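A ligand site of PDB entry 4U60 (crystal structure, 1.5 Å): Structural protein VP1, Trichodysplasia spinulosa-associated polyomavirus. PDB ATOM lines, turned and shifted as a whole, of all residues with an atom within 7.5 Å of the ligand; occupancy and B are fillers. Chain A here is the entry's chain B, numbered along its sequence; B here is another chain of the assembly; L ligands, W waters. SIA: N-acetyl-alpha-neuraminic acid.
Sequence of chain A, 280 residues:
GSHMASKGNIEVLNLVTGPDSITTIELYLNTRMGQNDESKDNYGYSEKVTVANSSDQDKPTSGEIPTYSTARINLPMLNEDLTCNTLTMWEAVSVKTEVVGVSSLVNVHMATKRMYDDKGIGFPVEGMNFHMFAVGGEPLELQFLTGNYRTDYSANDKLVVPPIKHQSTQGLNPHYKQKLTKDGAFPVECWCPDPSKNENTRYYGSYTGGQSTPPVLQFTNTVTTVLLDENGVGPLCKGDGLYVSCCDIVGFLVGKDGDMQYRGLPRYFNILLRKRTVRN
A nitrogen (N5) of the ligand sits at hydrogen-bond distance from the side-chain hydroxyl of Thr 50, 2.9 Å away. The backbone carbonyl oxygen of Val 51 sits at hydrogen-bond distance from an oxygen (O7) of the ligand (3.0 Å). The backbone carbonyl oxygen of Lys 59 sits at hydrogen-bond distance from an oxygen (O4) of the ligand, at 2.6 Å. NH1 of Arg 114 of chain B lies within hydrogen-bond range of O9 of the ligand, 2.9 Å away. N of Val 51 is in hydrogen-bond range of O9 of the ligand. N of Lys 59 sits at hydrogen-bond distance from O10 of the ligand, at 3.0 Å.
OE1 of Glu 64 lies within hydrogen-bond range of OG1 of Thr 50, 2.7 Å away. The side-chain carboxylate (OD1) of Asp 58 sits at hydrogen-bond distance from a ring nitrogen (ND1) of His 109 of chain B, at 2.8 Å. OG1 of Thr 61 sits at hydrogen-bond distance from OE1 of Glu 64. O of His 109 of chain B sits at hydrogen-bond distance from N of Ala 52. NH2 of Arg 114 of chain B is in hydrogen-bond range of O of Gly 120 of chain B (2.9 Å). The side-chain amide nitrogen (NE2) of Gln 57 lies within hydrogen-bond range of the side-chain hydroxyl (OG) of Ser 54 (2.7 Å). O of Asp 118 of chain B lies close to NH1 of Arg 114 of chain B (3.3 Å). NE2 of Gln 57 lies close to ND2 of Asn 53.
O of Gln 57 lies close to O10 of the ligand (3.1 Å). Merely in contact with the ligand: Ala 52, Asp 58, Pro 60, Thr 61 and His 109 of chain B. Ten residues have an atom within 4 Å of the ligand: Thr 50, Val 51, Ala 52, Gln 57, Asp 58, Lys 59, Pro 60, Thr 61, His 109 of chain B and Arg 114 of chain B.
Water W1 bridges an oxygen (O4) of the ligand (2.9 Å) and the backbone carbonyl oxygen (O) of Lys 59 (3.5 Å). Water W3 lies within hydrogen-bond range of the backbone NH of Asn 53 (2.8 Å), an oxygen (O10) of the ligand (3.0 Å) and the backbone carbonyl oxygen of Gln 57 (3.1 Å). Water W4 lies within hydrogen-bond range of O of Gln 57 (2.8 Å) and O4 of the ligand (3.2 Å).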
ATOM      1  N   VAL A  49      23.743   1.922 -26.498  1.00  0.00           N
ATOM      2  CA  VAL A  49      24.767   1.798 -25.485  1.00  0.00           C
ATOM      3  C   VAL A  49      24.147   1.887 -24.074  1.00  0.00           C
ATOM      4  O   VAL A  49      23.293   2.736 -23.807  1.00  0.00           O
ATOM      5  CB  VAL A  49      25.846   2.906 -25.659  1.00  0.00           C
ATOM      6  CG1 VAL A  49      26.787   2.946 -24.465  1.00  0.00           C
ATOM      7  CG2 VAL A  49      26.626   2.673 -26.946  1.00  0.00           C
ATOM      8  N   THR A  50      24.600   0.998 -23.192  1.00  0.00           N
ATOM      9  CA  THR A  50      24.201   1.029 -21.777  1.00  0.00           C
ATOM     10  C   THR A  50      25.461   1.203 -20.942  1.00  0.00           C
ATOM     11  O   THR A  50      26.568   1.016 -21.441  1.00  0.00           O
ATOM     12  CB  THR A  50      23.414  -0.232 -21.337  1.00  0.00           C
ATOM     13  OG1 THR A  50      24.275  -1.370 -21.316  1.00  0.00           O
ATOM     14  CG2 THR A  50      22.220  -0.470 -22.244  1.00  0.00           C
ATOM     15  N   VAL A  51      25.283   1.590 -19.684  1.00  0.00           N
ATOM     16  CA  VAL A  51      26.417   1.959 -18.858  1.00  0.00           C
ATOM     17  C   VAL A  51      26.361   1.177 -17.556  1.00  0.00           C
ATOM     18  O   VAL A  51      25.339   1.183 -16.858  1.00  0.00           O
ATOM     19  CB  VAL A  51      26.428   3.477 -18.609  1.00  0.00           C
ATOM     20  CG1 VAL A  51      27.516   3.875 -17.589  1.00  0.00           C
ATOM     21  CG2 VAL A  51      26.624   4.227 -19.929  1.00  0.00           C
ATOM     22  N   ALA A  52      27.449   0.506 -17.222  1.00  0.00           N
ATOM     23  CA  ALA A  52      27.538  -0.278 -15.983  1.00  0.00           C
ATOM     24  C   ALA A  52      27.242   0.517 -14.721  1.00  0.00           C
ATOM     25  O   ALA A  52      27.690   1.658 -14.560  1.00  0.00           O
ATOM     26  CB  ALA A  52      28.910  -0.913 -15.879  1.00  0.00           C
ATOM     27  N   ASN A  53      26.508  -0.105 -13.793  1.00  0.00           N
ATOM     28  CA  ASN A  53      26.247   0.508 -12.495  1.00  0.00           C
ATOM     29  C   ASN A  53      27.531   0.543 -11.665  1.00  0.00           C
ATOM     30  O   ASN A  53      27.731   1.455 -10.881  1.00  0.00           O
ATOM     31  CB  ASN A  53      25.105  -0.227 -11.794  1.00  0.00           C
ATOM     32  CG  ASN A  53      24.716   0.429 -10.485  1.00  0.00           C
ATOM     33  OD1 ASN A  53      24.237   1.568 -10.463  1.00  0.00           O
ATOM     34  ND2 ASN A  53      24.925  -0.273  -9.390  1.00  0.00           N
ATOM     35  N   SER A  54      28.397  -0.445 -11.844  1.00  0.00           N
ATOM     36  CA  SER A  54      29.688  -0.537 -11.178  1.00  0.00           C
ATOM     37  C   SER A  54      30.589  -1.427 -12.005  1.00  0.00           C
ATOM     38  O   SER A  54      30.098  -2.168 -12.860  1.00  0.00           O
ATOM     39  CB  SER A  54      29.545  -1.120  -9.775  1.00  0.00           C
ATOM     40  OG  SER A  54      29.048  -2.451  -9.853  1.00  0.00           O
ATOM     41  N   ASP A  56      32.028  -4.120 -11.258  1.00  0.00           N
ATOM     42  CA  ASP A  56      31.685  -5.521 -11.000  1.00  0.00           C
ATOM     43  C   ASP A  56      30.461  -5.981 -11.744  1.00  0.00           C
ATOM     44  O   ASP A  56      30.268  -7.179 -11.943  1.00  0.00           O
ATOM     45  CB  ASP A  56      31.411  -5.726  -9.501  1.00  0.00           C
ATOM     46  CG  ASP A  56      32.635  -5.580  -8.669  1.00  0.00           C
ATOM     47  OD1 ASP A  56      33.731  -5.547  -9.260  1.00  0.00           O
ATOM     48  OD2 ASP A  56      32.500  -5.487  -7.435  1.00  0.00           O
ATOM     49  N   GLN A  57      29.600  -5.044 -12.123  1.00  0.00           N
ATOM     50  CA  GLN A  57      28.321  -5.367 -12.723  1.00  0.00           C
ATOM     51  C   GLN A  57      28.328  -5.048 -14.227  1.00  0.00           C
ATOM     52  O   GLN A  57      27.281  -4.986 -14.853  1.00  0.00           O
ATOM     53  CB  GLN A  57      27.219  -4.560 -12.038  1.00  0.00           C
ATOM     54  CG  GLN A  57      26.958  -4.922 -10.589  1.00  0.00           C
ATOM     55  CD  GLN A  57      25.991  -3.967  -9.911  1.00  0.00           C
ATOM     56  OE1 GLN A  57      24.890  -4.346  -9.501  1.00  0.00           O
ATOM     57  NE2 GLN A  57      26.412  -2.726  -9.769  1.00  0.00           N
ATOM     58  N   ASP A  58      29.510  -4.927 -14.812  1.00  0.00           N
ATOM     59  CA  ASP A  58      29.679  -4.433 -16.169  1.00  0.00           C
ATOM     60  C   ASP A  58      29.407  -5.560 -17.169  1.00  0.00           C
ATOM     61  O   ASP A  58      30.246  -6.427 -17.376  1.00  0.00           O
ATOM     62  CB  ASP A  58      31.099  -3.874 -16.298  1.00  0.00           C
ATOM     63  CG  ASP A  58      31.359  -3.117 -17.601  1.00  0.00           C
ATOM     64  OD1 ASP A  58      30.523  -3.134 -18.524  1.00  0.00           O
ATOM     65  OD2 ASP A  58      32.438  -2.480 -17.661  1.00  0.00           O
ATOM     66  N   LYS A  59      28.215  -5.556 -17.736  1.00  0.00           N
ATOM     67  CA  LYS A  59      27.766  -6.614 -18.625  1.00  0.00           C
ATOM     68  C   LYS A  59      27.086  -5.971 -19.826  1.00  0.00           C
ATOM     69  O   LYS A  59      25.904  -5.638 -19.772  1.00  0.00           O
ATOM     70  CB  LYS A  59      26.776  -7.527 -17.905  1.00  0.00           C
ATOM     71  CG  LYS A  59      26.295  -8.705 -18.761  1.00  0.00           C
ATOM     72  CD  LYS A  59      25.328  -9.624 -18.040  1.00  0.00           C
ATOM     73  CE  LYS A  59      24.965 -10.810 -18.940  1.00  0.00           C
ATOM     74  NZ  LYS A  59      24.002 -11.725 -18.290  1.00  0.00           N
ATOM     75  N   PRO A  60      27.829  -5.779 -20.924  1.00  0.00           N
ATOM     76  CA  PRO A  60      27.186  -5.133 -22.073  1.00  0.00           C
ATOM     77  C   PRO A  60      26.015  -5.925 -22.604  1.00  0.00           C
ATOM     78  O   PRO A  60      26.039  -7.163 -22.558  1.00  0.00           O
ATOM     79  CB  PRO A  60      28.282  -5.074 -23.139  1.00  0.00           C
ATOM     80  CG  PRO A  60      29.407  -5.915 -22.626  1.00  0.00           C
ATOM     81  CD  PRO A  60      29.269  -5.973 -21.134  1.00  0.00           C
ATOM     82  N   THR A  61      24.992  -5.233 -23.039  1.00  0.00           N
ATOM     83  CA  THR A  61      23.846  -5.909 -23.650  1.00  0.00           C
ATOM     84  C   THR A  61      24.258  -6.546 -24.991  1.00  0.00           C
ATOM     85  O   THR A  61      25.257  -6.187 -25.597  1.00  0.00           O
ATOM     86  CB  THR A  61      22.665  -4.966 -23.892  1.00  0.00           C
ATOM     87  OG1 THR A  61      23.087  -3.924 -24.772  1.00  0.00           O
ATOM     88  CG2 THR A  61      22.158  -4.339 -22.592  1.00  0.00           C
ATOM     89  N   SER A  62      23.481  -7.531 -25.419  1.00  0.00           N
ATOM     90  CA  SER A  62      23.768  -8.185 -26.694  1.00  0.00           C
ATOM     91  C   SER A  62      23.625  -7.166 -27.819  1.00  0.00           C
ATOM     92  O   SER A  62      22.612  -6.478 -27.922  1.00  0.00           O
ATOM     93  CB  SER A  62      22.816  -9.372 -26.922  1.00  0.00           C
ATOM     94  OG  SER A  62      23.218 -10.086 -28.090  1.00  0.00           O
ATOM     95  N   GLU A  64      25.550  -4.394 -28.387  1.00  0.00           N
ATOM     96  CA  GLU A  64      26.021  -3.009 -28.171  1.00  0.00           C
ATOM     97  C   GLU A  64      27.519  -2.794 -28.359  1.00  0.00           C
ATOM     98  O   GLU A  64      27.983  -1.657 -28.191  1.00  0.00           O
ATOM     99  CB  GLU A  64      25.528  -2.424 -26.830  1.00  0.00           C
ATOM    100  CG  GLU A  64      26.282  -2.874 -25.584  1.00  0.00           C
ATOM    101  CD  GLU A  64      25.943  -2.039 -24.385  1.00  0.00           C
ATOM    102  OE1 GLU A  64      25.056  -2.493 -23.603  1.00  0.00           O
ATOM    103  OE2 GLU A  64      26.484  -0.918 -24.244  1.00  0.00           O
ATOM    104  N   THR A 151      34.599  -7.444 -17.158  1.00  0.00           N
ATOM    105  CA  THR A 151      33.514  -7.337 -18.140  1.00  0.00           C
ATOM    106  C   THR A 151      32.923  -8.723 -18.438  1.00  0.00           C
ATOM    107  O   THR A 151      33.647  -9.658 -18.724  1.00  0.00           O
ATOM    108  CB  THR A 151      33.995  -6.690 -19.450  1.00  0.00           C
ATOM    109  OG1 THR A 151      34.705  -5.495 -19.137  1.00  0.00           O
ATOM    110  CG2 THR A 151      32.819  -6.318 -20.333  1.00  0.00           C
ATOM    111  N   ASP A 152      31.599  -8.806 -18.360  1.00  0.00           N
ATOM    112  CA  ASP A 152      30.882 -10.044 -18.568  1.00  0.00           C
ATOM    113  C   ASP A 152      30.265 -10.005 -19.975  1.00  0.00           C
ATOM    114  O   ASP A 152      29.435  -9.147 -20.267  1.00  0.00           O
ATOM    115  CB  ASP A 152      29.797 -10.143 -17.502  1.00  0.00           C
ATOM    116  CG  ASP A 152      29.036 -11.446 -17.557  1.00  0.00           C
ATOM    117  OD1 ASP A 152      28.821 -11.960 -18.661  1.00  0.00           O
ATOM    118  OD2 ASP A 152      28.630 -11.940 -16.510  1.00  0.00           O
ATOM    119  N   ALA A 155      25.992 -12.042 -22.307  1.00  0.00           N
ATOM    120  CA  ALA A 155      24.753 -11.689 -23.013  1.00  0.00           C
ATOM    121  C   ALA A 155      24.798 -12.150 -24.484  1.00  0.00           C
ATOM    122  O   ALA A 155      23.755 -12.267 -25.121  1.00  0.00           O
ATOM    123  CB  ALA A 155      24.465 -10.197 -22.949  1.00  0.00           C
ATOM    124  N   VAL B 108      32.518   2.413 -24.028  1.00  0.00           N
ATOM    125  CA  VAL B 108      31.699   3.466 -23.426  1.00  0.00           C
ATOM    126  C   VAL B 108      30.583   2.892 -22.566  1.00  0.00           C
ATOM    127  O   VAL B 108      29.563   3.541 -22.308  1.00  0.00           O
ATOM    128  CB  VAL B 108      31.128   4.421 -24.499  1.00  0.00           C
ATOM    129  CG1 VAL B 108      32.272   5.241 -25.112  1.00  0.00           C
ATOM    130  CG2 VAL B 108      30.383   3.674 -25.576  1.00  0.00           C
ATOM    131  N   HIS B 109      30.765   1.658 -22.105  1.00  0.00           N
ATOM    132  CA  HIS B 109      29.802   1.046 -21.169  1.00  0.00           C
ATOM    133  C   HIS B 109      30.375   0.787 -19.786  1.00  0.00           C
ATOM    134  O   HIS B 109      29.674   0.196 -18.956  1.00  0.00           O
ATOM    135  CB  HIS B 109      29.209  -0.254 -21.718  1.00  0.00           C
ATOM    136  CG  HIS B 109      30.227  -1.282 -22.060  1.00  0.00           C
ATOM    137  ND1 HIS B 109      30.828  -2.091 -21.111  1.00  0.00           N
ATOM    138  CD2 HIS B 109      30.765  -1.638 -23.250  1.00  0.00           C
ATOM    139  CE1 HIS B 109      31.705  -2.872 -21.713  1.00  0.00           C
ATOM    140  NE2 HIS B 109      31.681  -2.628 -23.004  1.00  0.00           N
ATOM    141  N   MET B 110      31.611   1.231 -19.534  1.00  0.00           N
ATOM    142  CA  MET B 110      32.176   1.111 -18.181  1.00  0.00           C
ATOM    143  C   MET B 110      31.397   2.002 -17.214  1.00  0.00           C
ATOM    144  O   MET B 110      30.656   2.897 -17.616  1.00  0.00           O
ATOM    145  CB  MET B 110      33.668   1.447 -18.182  1.00  0.00           C
ATOM    146  CG  MET B 110      34.482   0.374 -18.892  1.00  0.00           C
ATOM    147  SD  MET B 110      36.249   0.623 -18.832  1.00  0.00           S
ATOM    148  CE  MET B 110      36.420   2.191 -19.631  1.00  0.00           C
ATOM    149  N   ALA B 111      31.551   1.740 -15.910  1.00  0.00           N
ATOM    150  CA  ALA B 111      30.848   2.493 -14.889  1.00  0.00           C
ATOM    151  C   ALA B 111      31.489   3.865 -14.768  1.00  0.00           C
ATOM    152  O   ALA B 111      32.471   4.055 -14.036  1.00  0.00           O
ATOM    153  CB  ALA B 111      30.884   1.726 -13.571  1.00  0.00           C
ATOM    154  N   ARG B 114      28.157   9.853 -17.591  1.00  0.00           N
ATOM    155  CA  ARG B 114      27.501   9.643 -18.889  1.00  0.00           C
ATOM    156  C   ARG B 114      27.058  10.929 -19.539  1.00  0.00           C
ATOM    157  O   ARG B 114      26.791  11.926 -18.874  1.00  0.00           O
ATOM    158  CB  ARG B 114      26.211   8.848 -18.781  1.00  0.00           C
ATOM    159  CG  ARG B 114      26.264   7.548 -18.068  1.00  0.00           C
ATOM    160  CD  ARG B 114      24.871   6.966 -18.000  1.00  0.00           C
ATOM    161  NE  ARG B 114      24.366   6.572 -19.332  1.00  0.00           N
ATOM    162  CZ  ARG B 114      23.516   5.582 -19.550  1.00  0.00           C
ATOM    163  NH1 ARG B 114      22.997   4.909 -18.521  1.00  0.00           N
ATOM    164  NH2 ARG B 114      23.186   5.257 -20.790  1.00  0.00           N
ATOM    165  N   ASP B 118      22.075  11.175 -18.396  1.00  0.00           N
ATOM    166  CA  ASP B 118      22.158   9.757 -18.023  1.00  0.00           C
ATOM    167  C   ASP B 118      21.522   8.805 -19.037  1.00  0.00           C
ATOM    168  O   ASP B 118      21.213   7.663 -18.696  1.00  0.00           O
ATOM    169  CB  ASP B 118      21.603   9.527 -16.610  1.00  0.00           C
ATOM    170  CG  ASP B 118      22.579   9.960 -15.549  1.00  0.00           C
ATOM    171  OD1 ASP B 118      23.774   9.677 -15.702  1.00  0.00           O
ATOM    172  OD2 ASP B 118      22.160  10.584 -14.544  1.00  0.00           O
ATOM    173  N   LYS B 119      21.345   9.266 -20.275  1.00  0.00           N
ATOM    174  CA  LYS B 119      20.804   8.444 -21.346  1.00  0.00           C
ATOM    175  C   LYS B 119      21.876   8.056 -22.384  1.00  0.00           C
ATOM    176  O   LYS B 119      21.730   7.042 -23.055  1.00  0.00           O
ATOM    177  CB  LYS B 119      19.641   9.162 -22.036  1.00  0.00           C
ATOM    178  CG  LYS B 119      18.428   9.355 -21.143  1.00  0.00           C
ATOM    179  CD  LYS B 119      17.954   8.030 -20.616  1.00  0.00           C
ATOM    180  N   GLY B 120      22.941   8.845 -22.487  1.00  0.00           N
ATOM    181  CA  GLY B 120      23.953   8.652 -23.509  1.00  0.00           C
ATOM    182  C   GLY B 120      25.094   7.738 -23.120  1.00  0.00           C
ATOM    183  O   GLY B 120      25.016   7.005 -22.116  1.00  0.00           O
ATOM    184  N   LYS B 256      31.525   7.580 -12.031  1.00  0.00           N
ATOM    185  CA  LYS B 256      30.169   8.096 -11.938  1.00  0.00           C
ATOM    186  C   LYS B 256      30.012   9.376 -11.146  1.00  0.00           C
ATOM    187  O   LYS B 256      29.180  10.184 -11.491  1.00  0.00           O
ATOM    188  CB  LYS B 256      29.237   7.067 -11.313  1.00  0.00           C
ATOM    189  CG  LYS B 256      29.185   5.799 -12.102  1.00  0.00           C
ATOM    190  CD  LYS B 256      27.883   5.082 -11.922  1.00  0.00           C
ATOM    191  CE  LYS B 256      27.688   4.114 -13.077  1.00  0.00           C
ATOM    192  NZ  LYS B 256      26.313   4.236 -13.568  1.00  0.00           N
HETATM  193  C1  SIA L   1      19.934  -3.239 -19.268  1.00  0.00           C
HETATM  194  C2  SIA L   1      20.487  -3.614 -17.911  1.00  0.00           C
HETATM  195  C3  SIA L   1      21.469  -4.795 -17.912  1.00  0.00           C
HETATM  196  C4  SIA L   1      22.818  -4.466 -18.600  1.00  0.00           C
HETATM  197  C5  SIA L   1      23.359  -3.162 -18.017  1.00  0.00           C
HETATM  198  C6  SIA L   1      22.294  -2.082 -18.049  1.00  0.00           C
HETATM  199  C7  SIA L   1      22.706  -0.717 -17.539  1.00  0.00           C
HETATM  200  C8  SIA L   1      21.543   0.273 -17.501  1.00  0.00           C
HETATM  201  C9  SIA L   1      21.988   1.730 -17.527  1.00  0.00           C
HETATM  202  C10 SIA L   1      25.812  -2.910 -18.303  1.00  0.00           C
HETATM  203  C11 SIA L   1      26.862  -2.372 -19.241  1.00  0.00           C
HETATM  204  N5  SIA L   1      24.563  -2.732 -18.730  1.00  0.00           N
HETATM  205  O1A SIA L   1      19.799  -4.153 -20.103  1.00  0.00           O
HETATM  206  O1B SIA L   1      19.549  -2.069 -19.494  1.00  0.00           O
HETATM  207  O2  SIA L   1      19.310  -3.918 -17.132  1.00  0.00           O
HETATM  208  O4  SIA L   1      23.751  -5.520 -18.351  1.00  0.00           O
HETATM  209  O6  SIA L   1      21.114  -2.514 -17.300  1.00  0.00           O
HETATM  210  O7  SIA L   1      23.289  -0.857 -16.241  1.00  0.00           O
HETATM  211  O8  SIA L   1      20.724   0.110 -18.655  1.00  0.00           O
HETATM  212  O9  SIA L   1      22.375   2.122 -18.881  1.00  0.00           O
HETATM  213  O10 SIA L   1      26.161  -3.455 -17.251  1.00  0.00           O
HETATM  214  O   HOH W   1      23.214  -7.795 -20.052  1.00  0.00           O
HETATM  215  O   HOH W   2      18.617   0.145 -21.136  1.00  0.00           O
HETATM  216  O   HOH W   3      25.366  -2.609 -14.507  1.00  0.00           O
HETATM  217  O   HOH W   4      24.641  -5.898 -15.314  1.00  0.00           O
